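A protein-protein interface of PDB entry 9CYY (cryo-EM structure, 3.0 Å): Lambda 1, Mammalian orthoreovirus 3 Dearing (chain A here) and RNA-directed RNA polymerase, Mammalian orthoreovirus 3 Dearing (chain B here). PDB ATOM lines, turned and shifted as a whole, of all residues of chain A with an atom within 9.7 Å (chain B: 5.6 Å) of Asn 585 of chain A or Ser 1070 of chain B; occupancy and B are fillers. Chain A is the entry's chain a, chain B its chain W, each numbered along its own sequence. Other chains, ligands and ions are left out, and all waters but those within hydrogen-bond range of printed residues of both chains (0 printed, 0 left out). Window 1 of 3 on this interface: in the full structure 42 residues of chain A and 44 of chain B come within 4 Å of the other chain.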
ATOM      1  N   PHE A 223      -8.991 -12.557   7.659  1.00  0.00           N
ATOM      2  CA  PHE A 223     -10.123 -13.113   8.396  1.00  0.00           C
ATOM      3  C   PHE A 223     -11.140 -13.741   7.451  1.00  0.00           C
ATOM      4  O   PHE A 223     -11.651 -14.840   7.706  1.00  0.00           O
ATOM      5  CB  PHE A 223     -10.773 -12.012   9.235  1.00  0.00           C
ATOM      6  CG  PHE A 223     -11.750 -12.515  10.254  1.00  0.00           C
ATOM      7  CD1 PHE A 223     -11.310 -13.150  11.401  1.00  0.00           C
ATOM      8  CD2 PHE A 223     -13.110 -12.338  10.072  1.00  0.00           C
ATOM      9  CE1 PHE A 223     -12.209 -13.606  12.344  1.00  0.00           C
ATOM     10  CE2 PHE A 223     -14.014 -12.793  11.011  1.00  0.00           C
ATOM     11  CZ  PHE A 223     -13.562 -13.426  12.148  1.00  0.00           C
ATOM     12  N   ILE A 224     -11.442 -13.055   6.348  1.00  0.00           N
ATOM     13  CA  ILE A 224     -12.436 -13.555   5.402  1.00  0.00           C
ATOM     14  C   ILE A 224     -11.958 -14.847   4.754  1.00  0.00           C
ATOM     15  O   ILE A 224     -12.729 -15.804   4.603  1.00  0.00           O
ATOM     16  CB  ILE A 224     -12.763 -12.478   4.353  1.00  0.00           C
ATOM     17  CG1 ILE A 224     -13.732 -11.452   4.938  1.00  0.00           C
ATOM     18  CG2 ILE A 224     -13.350 -13.105   3.100  1.00  0.00           C
ATOM     19  CD1 ILE A 224     -15.057 -12.043   5.351  1.00  0.00           C
ATOM     20  N   SER A 226      -9.832 -16.996   6.009  1.00  0.00           N
ATOM     21  CA  SER A 226      -9.855 -18.034   7.033  1.00  0.00           C
ATOM     22  C   SER A 226     -11.265 -18.569   7.239  1.00  0.00           C
ATOM     23  O   SER A 226     -11.465 -19.779   7.395  1.00  0.00           O
ATOM     24  CB  SER A 226      -9.289 -17.488   8.344  1.00  0.00           C
ATOM     25  OG  SER A 226      -9.380 -18.452   9.376  1.00  0.00           O
ATOM     26  N   TRP A 227     -12.259 -17.678   7.251  1.00  0.00           N
ATOM     27  CA  TRP A 227     -13.636 -18.136   7.407  1.00  0.00           C
ATOM     28  C   TRP A 227     -14.095 -18.948   6.203  1.00  0.00           C
ATOM     29  O   TRP A 227     -14.720 -20.002   6.362  1.00  0.00           O
ATOM     30  CB  TRP A 227     -14.576 -16.956   7.626  1.00  0.00           C
ATOM     31  CG  TRP A 227     -16.009 -17.383   7.682  1.00  0.00           C
ATOM     32  CD1 TRP A 227     -16.610 -18.100   8.674  1.00  0.00           C
ATOM     33  CD2 TRP A 227     -17.016 -17.146   6.693  1.00  0.00           C
ATOM     34  NE1 TRP A 227     -17.932 -18.309   8.372  1.00  0.00           N
ATOM     35  CE2 TRP A 227     -18.207 -17.736   7.160  1.00  0.00           C
ATOM     36  CE3 TRP A 227     -17.030 -16.486   5.461  1.00  0.00           C
ATOM     37  CZ2 TRP A 227     -19.396 -17.686   6.439  1.00  0.00           C
ATOM     38  CZ3 TRP A 227     -18.211 -16.438   4.747  1.00  0.00           C
ATOM     39  CH2 TRP A 227     -19.377 -17.034   5.238  1.00  0.00           C
ATOM     40  N   GLN A 228     -13.799 -18.474   4.991  1.00  0.00           N
ATOM     41  CA  GLN A 228     -14.298 -19.145   3.796  1.00  0.00           C
ATOM     42  C   GLN A 228     -13.645 -20.498   3.564  1.00  0.00           C
ATOM     43  O   GLN A 228     -14.277 -21.379   2.973  1.00  0.00           O
ATOM     44  CB  GLN A 228     -14.102 -18.265   2.562  1.00  0.00           C
ATOM     45  CG  GLN A 228     -14.941 -17.003   2.558  1.00  0.00           C
ATOM     46  CD  GLN A 228     -14.703 -16.154   1.328  1.00  0.00           C
ATOM     47  OE1 GLN A 228     -13.854 -16.473   0.496  1.00  0.00           O
ATOM     48  NE2 GLN A 228     -15.457 -15.070   1.202  1.00  0.00           N
ATOM     49  N   ASN A 229     -12.404 -20.692   4.007  1.00  0.00           N
ATOM     50  CA  ASN A 229     -11.728 -21.964   3.793  1.00  0.00           C
ATOM     51  C   ASN A 229     -12.120 -23.032   4.806  1.00  0.00           C
ATOM     52  O   ASN A 229     -11.474 -24.082   4.858  1.00  0.00           O
ATOM     53  CB  ASN A 229     -10.211 -21.762   3.812  1.00  0.00           C
ATOM     54  CG  ASN A 229      -9.683 -21.234   2.495  1.00  0.00           C
ATOM     55  OD1 ASN A 229     -10.005 -20.117   2.089  1.00  0.00           O
ATOM     56  ND2 ASN A 229      -8.874 -22.037   1.817  1.00  0.00           N
ATOM     57  N   HIS A 230     -13.154 -22.797   5.607  1.00  0.00           N
ATOM     58  CA  HIS A 230     -13.592 -23.802   6.563  1.00  0.00           C
ATOM     59  C   HIS A 230     -14.353 -24.912   5.841  1.00  0.00           C
ATOM     60  O   HIS A 230     -15.114 -24.638   4.909  1.00  0.00           O
ATOM     61  CB  HIS A 230     -14.474 -23.167   7.637  1.00  0.00           C
ATOM     62  CG  HIS A 230     -14.840 -24.099   8.749  1.00  0.00           C
ATOM     63  ND1 HIS A 230     -15.948 -24.916   8.702  1.00  0.00           N
ATOM     64  CD2 HIS A 230     -14.241 -24.346   9.936  1.00  0.00           C
ATOM     65  CE1 HIS A 230     -16.017 -25.623   9.815  1.00  0.00           C
ATOM     66  NE2 HIS A 230     -14.993 -25.296  10.581  1.00  0.00           N
ATOM     67  N   PRO A 231     -14.170 -26.174   6.247  1.00  0.00           N
ATOM     68  CA  PRO A 231     -14.807 -27.282   5.509  1.00  0.00           C
ATOM     69  C   PRO A 231     -16.324 -27.212   5.442  1.00  0.00           C
ATOM     70  O   PRO A 231     -16.902 -27.397   4.365  1.00  0.00           O
ATOM     71  CB  PRO A 231     -14.334 -28.518   6.286  1.00  0.00           C
ATOM     72  CG  PRO A 231     -13.068 -28.096   6.932  1.00  0.00           C
ATOM     73  CD  PRO A 231     -13.258 -26.659   7.294  1.00  0.00           C
ATOM     74  N   ILE A 232     -16.989 -26.958   6.570  1.00  0.00           N
ATOM     75  CA  ILE A 232     -18.449 -26.932   6.581  1.00  0.00           C
ATOM     76  C   ILE A 232     -18.971 -25.746   5.780  1.00  0.00           C
ATOM     77  O   ILE A 232     -20.006 -25.841   5.109  1.00  0.00           O
ATOM     78  CB  ILE A 232     -18.975 -26.918   8.026  1.00  0.00           C
ATOM     79  CG1 ILE A 232     -18.281 -27.999   8.854  1.00  0.00           C
ATOM     80  CG2 ILE A 232     -20.479 -27.120   8.046  1.00  0.00           C
ATOM     81  CD1 ILE A 232     -18.492 -29.400   8.326  1.00  0.00           C
ATOM     82  N   VAL A 233     -18.272 -24.613   5.840  1.00  0.00           N
ATOM     83  CA  VAL A 233     -18.699 -23.431   5.096  1.00  0.00           C
ATOM     84  C   VAL A 233     -18.649 -23.697   3.596  1.00  0.00           C
ATOM     85  O   VAL A 233     -19.422 -23.117   2.821  1.00  0.00           O
ATOM     86  CB  VAL A 233     -17.839 -22.217   5.494  1.00  0.00           C
ATOM     87  CG1 VAL A 233     -18.239 -20.983   4.701  1.00  0.00           C
ATOM     88  CG2 VAL A 233     -17.959 -21.954   6.985  1.00  0.00           C
ATOM     89  N   GLN A 234     -17.755 -24.590   3.164  1.00  0.00           N
ATOM     90  CA  GLN A 234     -17.619 -24.876   1.738  1.00  0.00           C
ATOM     91  C   GLN A 234     -18.920 -25.409   1.150  1.00  0.00           C
ATOM     92  O   GLN A 234     -19.337 -24.987   0.065  1.00  0.00           O
ATOM     93  CB  GLN A 234     -16.485 -25.873   1.506  1.00  0.00           C
ATOM     94  CG  GLN A 234     -15.105 -25.340   1.839  1.00  0.00           C
ATOM     95  CD  GLN A 234     -14.635 -24.284   0.861  1.00  0.00           C
ATOM     96  OE1 GLN A 234     -14.881 -24.382  -0.341  1.00  0.00           O
ATOM     97  NE2 GLN A 234     -13.955 -23.265   1.372  1.00  0.00           N
ATOM     98  N   SER A 236     -22.847 -25.821   2.157  1.00  0.00           N
ATOM     99  CA  SER A 236     -23.947 -25.484   3.054  1.00  0.00           C
ATOM    100  C   SER A 236     -24.901 -24.568   2.303  1.00  0.00           C
ATOM    101  O   SER A 236     -24.515 -23.909   1.332  1.00  0.00           O
ATOM    102  CB  SER A 236     -23.454 -24.805   4.336  1.00  0.00           C
ATOM    103  OG  SER A 236     -22.496 -23.802   4.045  1.00  0.00           O
ATOM    104  N   ARG A 582      -9.359 -25.971  20.737  1.00  0.00           N
ATOM    105  CA  ARG A 582     -10.561 -25.171  20.540  1.00  0.00           C
ATOM    106  C   ARG A 582     -10.915 -25.169  19.058  1.00  0.00           C
ATOM    107  O   ARG A 582     -10.213 -24.543  18.255  1.00  0.00           O
ATOM    108  CB  ARG A 582     -10.361 -23.747  21.056  1.00  0.00           C
ATOM    109  CG  ARG A 582      -9.754 -23.678  22.445  1.00  0.00           C
ATOM    110  CD  ARG A 582      -9.689 -22.251  22.961  1.00  0.00           C
ATOM    111  NE  ARG A 582     -11.001 -21.753  23.360  1.00  0.00           N
ATOM    112  CZ  ARG A 582     -11.594 -20.694  22.829  1.00  0.00           C
ATOM    113  NH1 ARG A 582     -11.018 -19.987  21.872  1.00  0.00           N
ATOM    114  NH2 ARG A 582     -12.796 -20.336  23.269  1.00  0.00           N
ATOM    115  N   PRO A 583     -11.993 -25.848  18.665  1.00  0.00           N
ATOM    116  CA  PRO A 583     -12.271 -26.040  17.237  1.00  0.00           C
ATOM    117  C   PRO A 583     -12.474 -24.721  16.505  1.00  0.00           C
ATOM    118  O   PRO A 583     -13.010 -23.756  17.051  1.00  0.00           O
ATOM    119  CB  PRO A 583     -13.554 -26.877  17.239  1.00  0.00           C
ATOM    120  CG  PRO A 583     -13.555 -27.553  18.561  1.00  0.00           C
ATOM    121  CD  PRO A 583     -12.966 -26.555  19.509  1.00  0.00           C
ATOM    122  N   SER A 584     -12.027 -24.694  15.252  1.00  0.00           N
ATOM    123  CA  SER A 584     -12.220 -23.535  14.396  1.00  0.00           C
ATOM    124  C   SER A 584     -13.702 -23.310  14.132  1.00  0.00           C
ATOM    125  O   SER A 584     -14.438 -24.248  13.812  1.00  0.00           O
ATOM    126  CB  SER A 584     -11.478 -23.726  13.075  1.00  0.00           C
ATOM    127  OG  SER A 584     -11.742 -22.661  12.181  1.00  0.00           O
ATOM    128  N   ASN A 585     -14.137 -22.060  14.286  1.00  0.00           N
ATOM    129  CA  ASN A 585     -15.493 -21.590  14.019  1.00  0.00           C
ATOM    130  C   ASN A 585     -16.526 -22.185  14.970  1.00  0.00           C
ATOM    131  O   ASN A 585     -17.712 -21.856  14.851  1.00  0.00           O
ATOM    132  CB  ASN A 585     -15.924 -21.864  12.570  1.00  0.00           C
ATOM    133  CG  ASN A 585     -17.001 -20.913  12.088  1.00  0.00           C
ATOM    134  OD1 ASN A 585     -17.439 -20.028  12.820  1.00  0.00           O
ATOM    135  ND2 ASN A 585     -17.430 -21.091  10.845  1.00  0.00           N
ATOM    136  N   SER A 586     -16.121 -23.039  15.911  1.00  0.00           N
ATOM    137  CA  SER A 586     -17.020 -23.639  16.897  1.00  0.00           C
ATOM    138  C   SER A 586     -18.151 -24.413  16.212  1.00  0.00           C
ATOM    139  O   SER A 586     -19.324 -24.057  16.288  1.00  0.00           O
ATOM    140  CB  SER A 586     -17.577 -22.570  17.842  1.00  0.00           C
ATOM    141  OG  SER A 586     -16.536 -21.908  18.535  1.00  0.00           O
ATOM    142  N   ASP A 587     -17.755 -25.480  15.520  1.00  0.00           N
ATOM    143  CA  ASP A 587     -18.687 -26.301  14.753  1.00  0.00           C
ATOM    144  C   ASP A 587     -19.264 -27.471  15.547  1.00  0.00           C
ATOM    145  O   ASP A 587     -20.486 -27.619  15.617  1.00  0.00           O
ATOM    146  CB  ASP A 587     -18.006 -26.794  13.467  1.00  0.00           C
ATOM    147  CG  ASP A 587     -16.804 -27.686  13.734  1.00  0.00           C
ATOM    148  OD1 ASP A 587     -16.462 -27.898  14.916  1.00  0.00           O
ATOM    149  OD2 ASP A 587     -16.196 -28.169  12.757  1.00  0.00           O
ATOM    150  N   PHE A 588     -18.413 -28.328  16.118  1.00  0.00           N
ATOM    151  CA  PHE A 588     -18.841 -29.412  17.012  1.00  0.00           C
ATOM    152  C   PHE A 588     -19.887 -30.331  16.379  1.00  0.00           C
ATOM    153  O   PHE A 588     -20.569 -31.084  17.077  1.00  0.00           O
ATOM    154  CB  PHE A 588     -19.365 -28.857  18.337  1.00  0.00           C
ATOM    155  CG  PHE A 588     -18.312 -28.199  19.176  1.00  0.00           C
ATOM    156  CD1 PHE A 588     -17.271 -28.940  19.702  1.00  0.00           C
ATOM    157  CD2 PHE A 588     -18.364 -26.841  19.442  1.00  0.00           C
ATOM    158  CE1 PHE A 588     -16.302 -28.344  20.478  1.00  0.00           C
ATOM    159  CE2 PHE A 588     -17.393 -26.237  20.218  1.00  0.00           C
ATOM    160  CZ  PHE A 588     -16.360 -26.990  20.735  1.00  0.00           C
ATOM    161  N   SER A 589     -20.025 -30.292  15.053  1.00  0.00           N
ATOM    162  CA  SER A 589     -20.998 -31.127  14.362  1.00  0.00           C
ATOM    163  C   SER A 589     -20.362 -32.221  13.520  1.00  0.00           C
ATOM    164  O   SER A 589     -21.060 -33.169  13.133  1.00  0.00           O
ATOM    165  CB  SER A 589     -21.902 -30.264  13.471  1.00  0.00           C
ATOM    166  OG  SER A 589     -21.169 -29.693  12.403  1.00  0.00           O
ATOM    167  N   SER A 590     -19.062 -32.121  13.238  1.00  0.00           N
ATOM    168  CA  SER A 590     -18.392 -33.137  12.439  1.00  0.00           C
ATOM    169  C   SER A 590     -18.466 -34.506  13.096  1.00  0.00           C
ATOM    170  O   SER A 590     -18.484 -35.521  12.397  1.00  0.00           O
ATOM    171  CB  SER A 590     -16.938 -32.740  12.197  1.00  0.00           C
ATOM    172  OG  SER A 590     -16.853 -31.423  11.684  1.00  0.00           O
ATOM    173  N   ASP A 878     -13.778 -32.019  10.085  1.00  0.00           N
ATOM    174  CA  ASP A 878     -12.780 -31.371  10.925  1.00  0.00           C
ATOM    175  C   ASP A 878     -12.320 -32.335  12.011  1.00  0.00           C
ATOM    176  O   ASP A 878     -13.146 -32.931  12.710  1.00  0.00           O
ATOM    177  CB  ASP A 878     -13.345 -30.096  11.553  1.00  0.00           C
ATOM    178  CG  ASP A 878     -12.276 -29.240  12.199  1.00  0.00           C
ATOM    179  OD1 ASP A 878     -11.085 -29.599  12.104  1.00  0.00           O
ATOM    180  OD2 ASP A 878     -12.628 -28.206  12.805  1.00  0.00           O
ATOM    181  N   ARG A 880     -10.412 -31.610  14.721  1.00  0.00           N
ATOM    182  CA  ARG A 880     -10.360 -31.045  16.065  1.00  0.00           C
ATOM    183  C   ARG A 880     -11.672 -31.259  16.809  1.00  0.00           C
ATOM    184  O   ARG A 880     -11.674 -31.628  17.990  1.00  0.00           O
ATOM    185  CB  ARG A 880     -10.013 -29.560  15.969  1.00  0.00           C
ATOM    186  CG  ARG A 880      -8.607 -29.327  15.440  1.00  0.00           C
ATOM    187  CD  ARG A 880      -8.255 -27.858  15.308  1.00  0.00           C
ATOM    188  NE  ARG A 880      -8.174 -27.166  16.587  1.00  0.00           N
ATOM    189  CZ  ARG A 880      -8.039 -25.854  16.713  1.00  0.00           C
ATOM    190  NH1 ARG A 880      -7.974 -25.061  15.655  1.00  0.00           N
ATOM    191  NH2 ARG A 880      -7.967 -25.321  17.929  1.00  0.00           N
ATOM    192  N   ALA A 881     -12.800 -31.047  16.128  1.00  0.00           N
ATOM    193  CA  ALA A 881     -14.100 -31.263  16.754  1.00  0.00           C
ATOM    194  C   ALA A 881     -14.288 -32.724  17.137  1.00  0.00           C
ATOM    195  O   ALA A 881     -14.803 -33.033  18.218  1.00  0.00           O
ATOM    196  CB  ALA A 881     -15.215 -30.804  15.816  1.00  0.00           C
ATOM    197  N   TYR B 310     -21.865 -23.835  22.951  1.00  0.00           N
ATOM    198  CA  TYR B 310     -22.441 -23.554  21.641  1.00  0.00           C
ATOM    199  C   TYR B 310     -22.034 -24.620  20.629  1.00  0.00           C
ATOM    200  O   TYR B 310     -20.841 -24.855  20.414  1.00  0.00           O
ATOM    201  CB  TYR B 310     -21.982 -22.164  21.198  1.00  0.00           C
ATOM    202  CG  TYR B 310     -22.093 -21.852  19.727  1.00  0.00           C
ATOM    203  CD1 TYR B 310     -23.288 -21.413  19.174  1.00  0.00           C
ATOM    204  CD2 TYR B 310     -20.995 -21.982  18.889  1.00  0.00           C
ATOM    205  CE1 TYR B 310     -23.385 -21.117  17.827  1.00  0.00           C
ATOM    206  CE2 TYR B 310     -21.085 -21.692  17.544  1.00  0.00           C
ATOM    207  CZ  TYR B 310     -22.281 -21.259  17.020  1.00  0.00           C
ATOM    208  OH  TYR B 310     -22.366 -20.971  15.679  1.00  0.00           O
ATOM    209  N   ARG B1067      -7.109 -12.979  14.117  1.00  0.00           N
ATOM    210  CA  ARG B1067      -7.629 -14.087  14.906  1.00  0.00           C
ATOM    211  C   ARG B1067      -8.389 -15.053  14.000  1.00  0.00           C
ATOM    212  O   ARG B1067      -8.381 -14.937  12.772  1.00  0.00           O
ATOM    213  CB  ARG B1067      -8.515 -13.569  16.035  1.00  0.00           C
ATOM    214  CG  ARG B1067      -7.781 -13.276  17.327  1.00  0.00           C
ATOM    215  CD  ARG B1067      -8.752 -13.169  18.489  1.00  0.00           C
ATOM    216  NE  ARG B1067      -9.674 -14.297  18.531  1.00  0.00           N
ATOM    217  CZ  ARG B1067     -10.379 -14.649  19.598  1.00  0.00           C
ATOM    218  NH1 ARG B1067     -10.306 -13.967  20.728  1.00  0.00           N
ATOM    219  NH2 ARG B1067     -11.174 -15.712  19.527  1.00  0.00           N
ATOM    220  N   GLU B1068      -9.060 -16.019  14.611  1.00  0.00           N
ATOM    221  CA  GLU B1068      -9.854 -17.011  13.914  1.00  0.00           C
ATOM    222  C   GLU B1068     -11.330 -16.820  14.247  1.00  0.00           C
ATOM    223  O   GLU B1068     -11.673 -16.511  15.392  1.00  0.00           O
ATOM    224  CB  GLU B1068      -9.406 -18.425  14.307  1.00  0.00           C
ATOM    225  CG  GLU B1068      -8.019 -18.804  13.847  1.00  0.00           C
ATOM    226  CD  GLU B1068      -7.619 -20.182  14.332  1.00  0.00           C
ATOM    227  OE1 GLU B1068      -8.344 -20.747  15.174  1.00  0.00           O
ATOM    228  OE2 GLU B1068      -6.570 -20.692  13.895  1.00  0.00           O
ATOM    229  N   PRO B1069     -12.225 -16.969  13.271  1.00  0.00           N
ATOM    230  CA  PRO B1069     -13.650 -16.725  13.530  1.00  0.00           C
ATOM    231  C   PRO B1069     -14.190 -17.592  14.658  1.00  0.00           C
ATOM    232  O   PRO B1069     -13.861 -18.774  14.773  1.00  0.00           O
ATOM    233  CB  PRO B1069     -14.309 -17.070  12.192  1.00  0.00           C
ATOM    234  CG  PRO B1069     -13.251 -16.817  11.186  1.00  0.00           C
ATOM    235  CD  PRO B1069     -11.963 -17.213  11.843  1.00  0.00           C
ATOM    236  N   SER B1070     -15.028 -16.989  15.499  1.00  0.00           N
ATOM    237  CA  SER B1070     -15.658 -17.685  16.612  1.00  0.00           C
ATOM    238  C   SER B1070     -17.123 -18.007  16.361  1.00  0.00           C
ATOM    239  O   SER B1070     -17.634 -18.976  16.931  1.00  0.00           O
ATOM    240  CB  SER B1070     -15.537 -16.852  17.894  1.00  0.00           C
ATOM    241  OG  SER B1070     -14.181 -16.665  18.254  1.00  0.00           O
ATOM    242  N   VAL B1071     -17.807 -17.223  15.530  1.00  0.00           N
ATOM    243  CA  VAL B1071     -19.214 -17.450  15.222  1.00  0.00           C
ATOM    244  C   VAL B1071     -19.373 -17.308  13.716  1.00  0.00           C
ATOM    245  O   VAL B1071     -18.637 -16.562  13.070  1.00  0.00           O
ATOM    246  CB  VAL B1071     -20.124 -16.459  15.995  1.00  0.00           C
ATOM    247  CG1 VAL B1071     -21.583 -16.623  15.599  1.00  0.00           C
ATOM    248  CG2 VAL B1071     -19.962 -16.639  17.494  1.00  0.00           C
ATOM    249  N   ASP B1072     -20.330 -18.039  13.150  1.00  0.00           N
ATOM    250  CA  ASP B1072     -20.594 -17.939  11.722  1.00  0.00           C
ATOM    251  C   ASP B1072     -21.034 -16.525  11.360  1.00  0.00           C
ATOM    252  O   ASP B1072     -21.742 -15.856  12.116  1.00  0.00           O
ATOM    253  CB  ASP B1072     -21.666 -18.945  11.306  1.00  0.00           C
ATOM    254  CG  ASP B1072     -21.870 -18.987   9.807  1.00  0.00           C
ATOM    255  OD1 ASP B1072     -20.900 -18.725   9.068  1.00  0.00           O
ATOM    256  OD2 ASP B1072     -23.002 -19.277   9.367  1.00  0.00           O
ATOM    257  N   MET B1092     -17.571  -8.517  17.158  1.00  0.00           N
ATOM    258  CA  MET B1092     -18.348  -9.609  17.725  1.00  0.00           C
ATOM    259  C   MET B1092     -18.015 -10.934  17.052  1.00  0.00           C
ATOM    260  O   MET B1092     -17.810 -11.947  17.728  1.00  0.00           O
ATOM    261  CB  MET B1092     -19.838  -9.295  17.609  1.00  0.00           C
ATOM    262  CG  MET B1092     -20.742 -10.304  18.275  1.00  0.00           C
ATOM    263  SD  MET B1092     -22.469  -9.834  18.093  1.00  0.00           S
ATOM    264  CE  MET B1092     -22.555  -8.436  19.209  1.00  0.00           C
ATOM    265  N   VAL B1093     -17.934 -10.948  15.718  1.00  0.00           N
ATOM    266  CA  VAL B1093     -17.600 -12.193  15.027  1.00  0.00           C
ATOM    267  C   VAL B1093     -16.147 -12.596  15.214  1.00  0.00           C
ATOM    268  O   VAL B1093     -15.803 -13.758  14.966  1.00  0.00           O
ATOM    269  CB  VAL B1093     -17.906 -12.118  13.520  1.00  0.00           C
ATOM    270  CG1 VAL B1093     -19.354 -11.724  13.292  1.00  0.00           C
ATOM    271  CG2 VAL B1093     -16.964 -11.151  12.828  1.00  0.00           C
ATOM    272  N   SER B1094     -15.282 -11.678  15.647  1.00  0.00           N
ATOM    273  CA  SER B1094     -13.891 -12.011  15.928  1.00  0.00           C
ATOM    274  C   SER B1094     -13.684 -12.528  17.345  1.00  0.00           C
ATOM    275  O   SER B1094     -12.921 -13.476  17.550  1.00  0.00           O
ATOM    276  CB  SER B1094     -13.002 -10.786  15.687  1.00  0.00           C
ATOM    277  OG  SER B1094     -13.077 -10.363  14.339  1.00  0.00           O
ATOM    278  N   VAL B1095     -14.350 -11.930  18.330  1.00  0.00           N
ATOM    279  CA  VAL B1095     -14.126 -12.332  19.713  1.00  0.00           C
ATOM    280  C   VAL B1095     -15.135 -13.377  20.185  1.00  0.00           C
ATOM    281  O   VAL B1095     -14.743 -14.385  20.779  1.00  0.00           O
ATOM    282  CB  VAL B1095     -14.145 -11.099  20.633  1.00  0.00           C
ATOM    283  CG1 VAL B1095     -13.821 -11.501  22.059  1.00  0.00           C
ATOM    284  CG2 VAL B1095     -13.161 -10.058  20.134  1.00  0.00           C
ATOM    285  N   GLY B1096     -16.423 -13.165  19.935  1.00  0.00           N
ATOM    286  CA  GLY B1096     -17.441 -14.093  20.357  1.00  0.00           C
ATOM    287  C   GLY B1096     -18.205 -13.594  21.564  1.00  0.00           C
ATOM    288  O   GLY B1096     -17.639 -13.000  22.487  1.00  0.00           O
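CD1 of Phe 223 of chain A touches O of Arg 1067 of chain B, at 3.7 Å.
Phe 223 of chain A touches Glu 1068 of chain B.
Phe 223 of chain A touches Val 1093 of chain B.
Phe 223 of chain A touches Ser 1094 of chain B.
Ser 226 of chain A touches Pro 1069 of chain B (OG to CD, 3.8 Å).
C of Val 1071 of chain B touches OD1 of Asn 585 of chain A, at 3.5 Å.
Asp 1072 of chain B touches Asn 585 of chain A (N to OD1, 3.5 Å).
Tyr 310 of chain B touches Ser 586 of chain A (CE2 to O, 3.2 Å).
Ser 586 of chain A touches Ser 1070 of chain B (OG to O, 3.5 Å).
Tyr 310 of chain B touches Phe 588 of chain A (O to CD2, 3.3 Å).
O of Pro 1069 of chain B lies within hydrogen-bond range of N of Asn 585 of chain A.
The indole nitrogen of Trp 227 of chain A lies within hydrogen-bond range of the side-chain carboxylate of Asp 1072 of chain B (3.1 Å).
N of Ser 1070 of chain B lies within hydrogen-bond range of O of Val 1093 of chain B (3.4 Å).
The guanidinium group (NH2) of Arg 1067 of chain B is in hydrogen-bond range of the side-chain hydroxyl (OG) of Ser 1070 of chain B (3.4 Å).
NH2 of Arg 1067 of chain B lies within hydrogen-bond range of O of Ser 1094 of chain B (3.5 Å).
O of Val 1095 of chain B sits at hydrogen-bond distance from OG of Ser 1070 of chain B (3.4 Å).
Of the 24 printed residues of chain A, 6 touch a printed residue of chain B.
Hydrophobic or aromatic side chains of chain A that line the printed part of chain B: Phe 223, Trp 227 and Phe 588.
Printed residues of chain B that touch a printed residue of chain A: Tyr 310, Arg 1067, Glu 1068, Pro 1069, Ser 1070, Val 1071, Asp 1072, Val 1093 and Ser 1094.
Among the printed residues, 15 pairs touch across the chains.
Among the printed residues, no Asp or Glu carboxylate lies within 4 Å of a Lys or Arg side-chain nitrogen of the other chain.
His 230 of chain A touches none of the printed residues of chain B.
Of the printed residues of chain B, Asn 585 of chain A touches Pro 1069 (3.3 Å), Ser 1070 (3.6 Å), Val 1071 (3.5 Å) and Asp 1072 (3.5 Å).
Of the printed residues of chain B, Phe 588 of chain A touches Tyr 310 (3.3 Å).
Of the printed residues of chain A, Arg 1067 of chain B touches Phe 223.
Of chain A, only Phe 223, Ser 226, Trp 227 and Asn 585 come within 4 Å of Pro 1069 of chain B.
Of chain A, only Asn 585 and Ser 586 come within 4 Å of Ser 1070 of chain B.
Val 1071 of chain B touches just one residue of chain A: Asn 585.
Of the printed residues of chain A, Val 1093 of chain B touches Phe 223.
Of the printed residues of chain A, Ser 1094 of chain B touches Phe 223.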
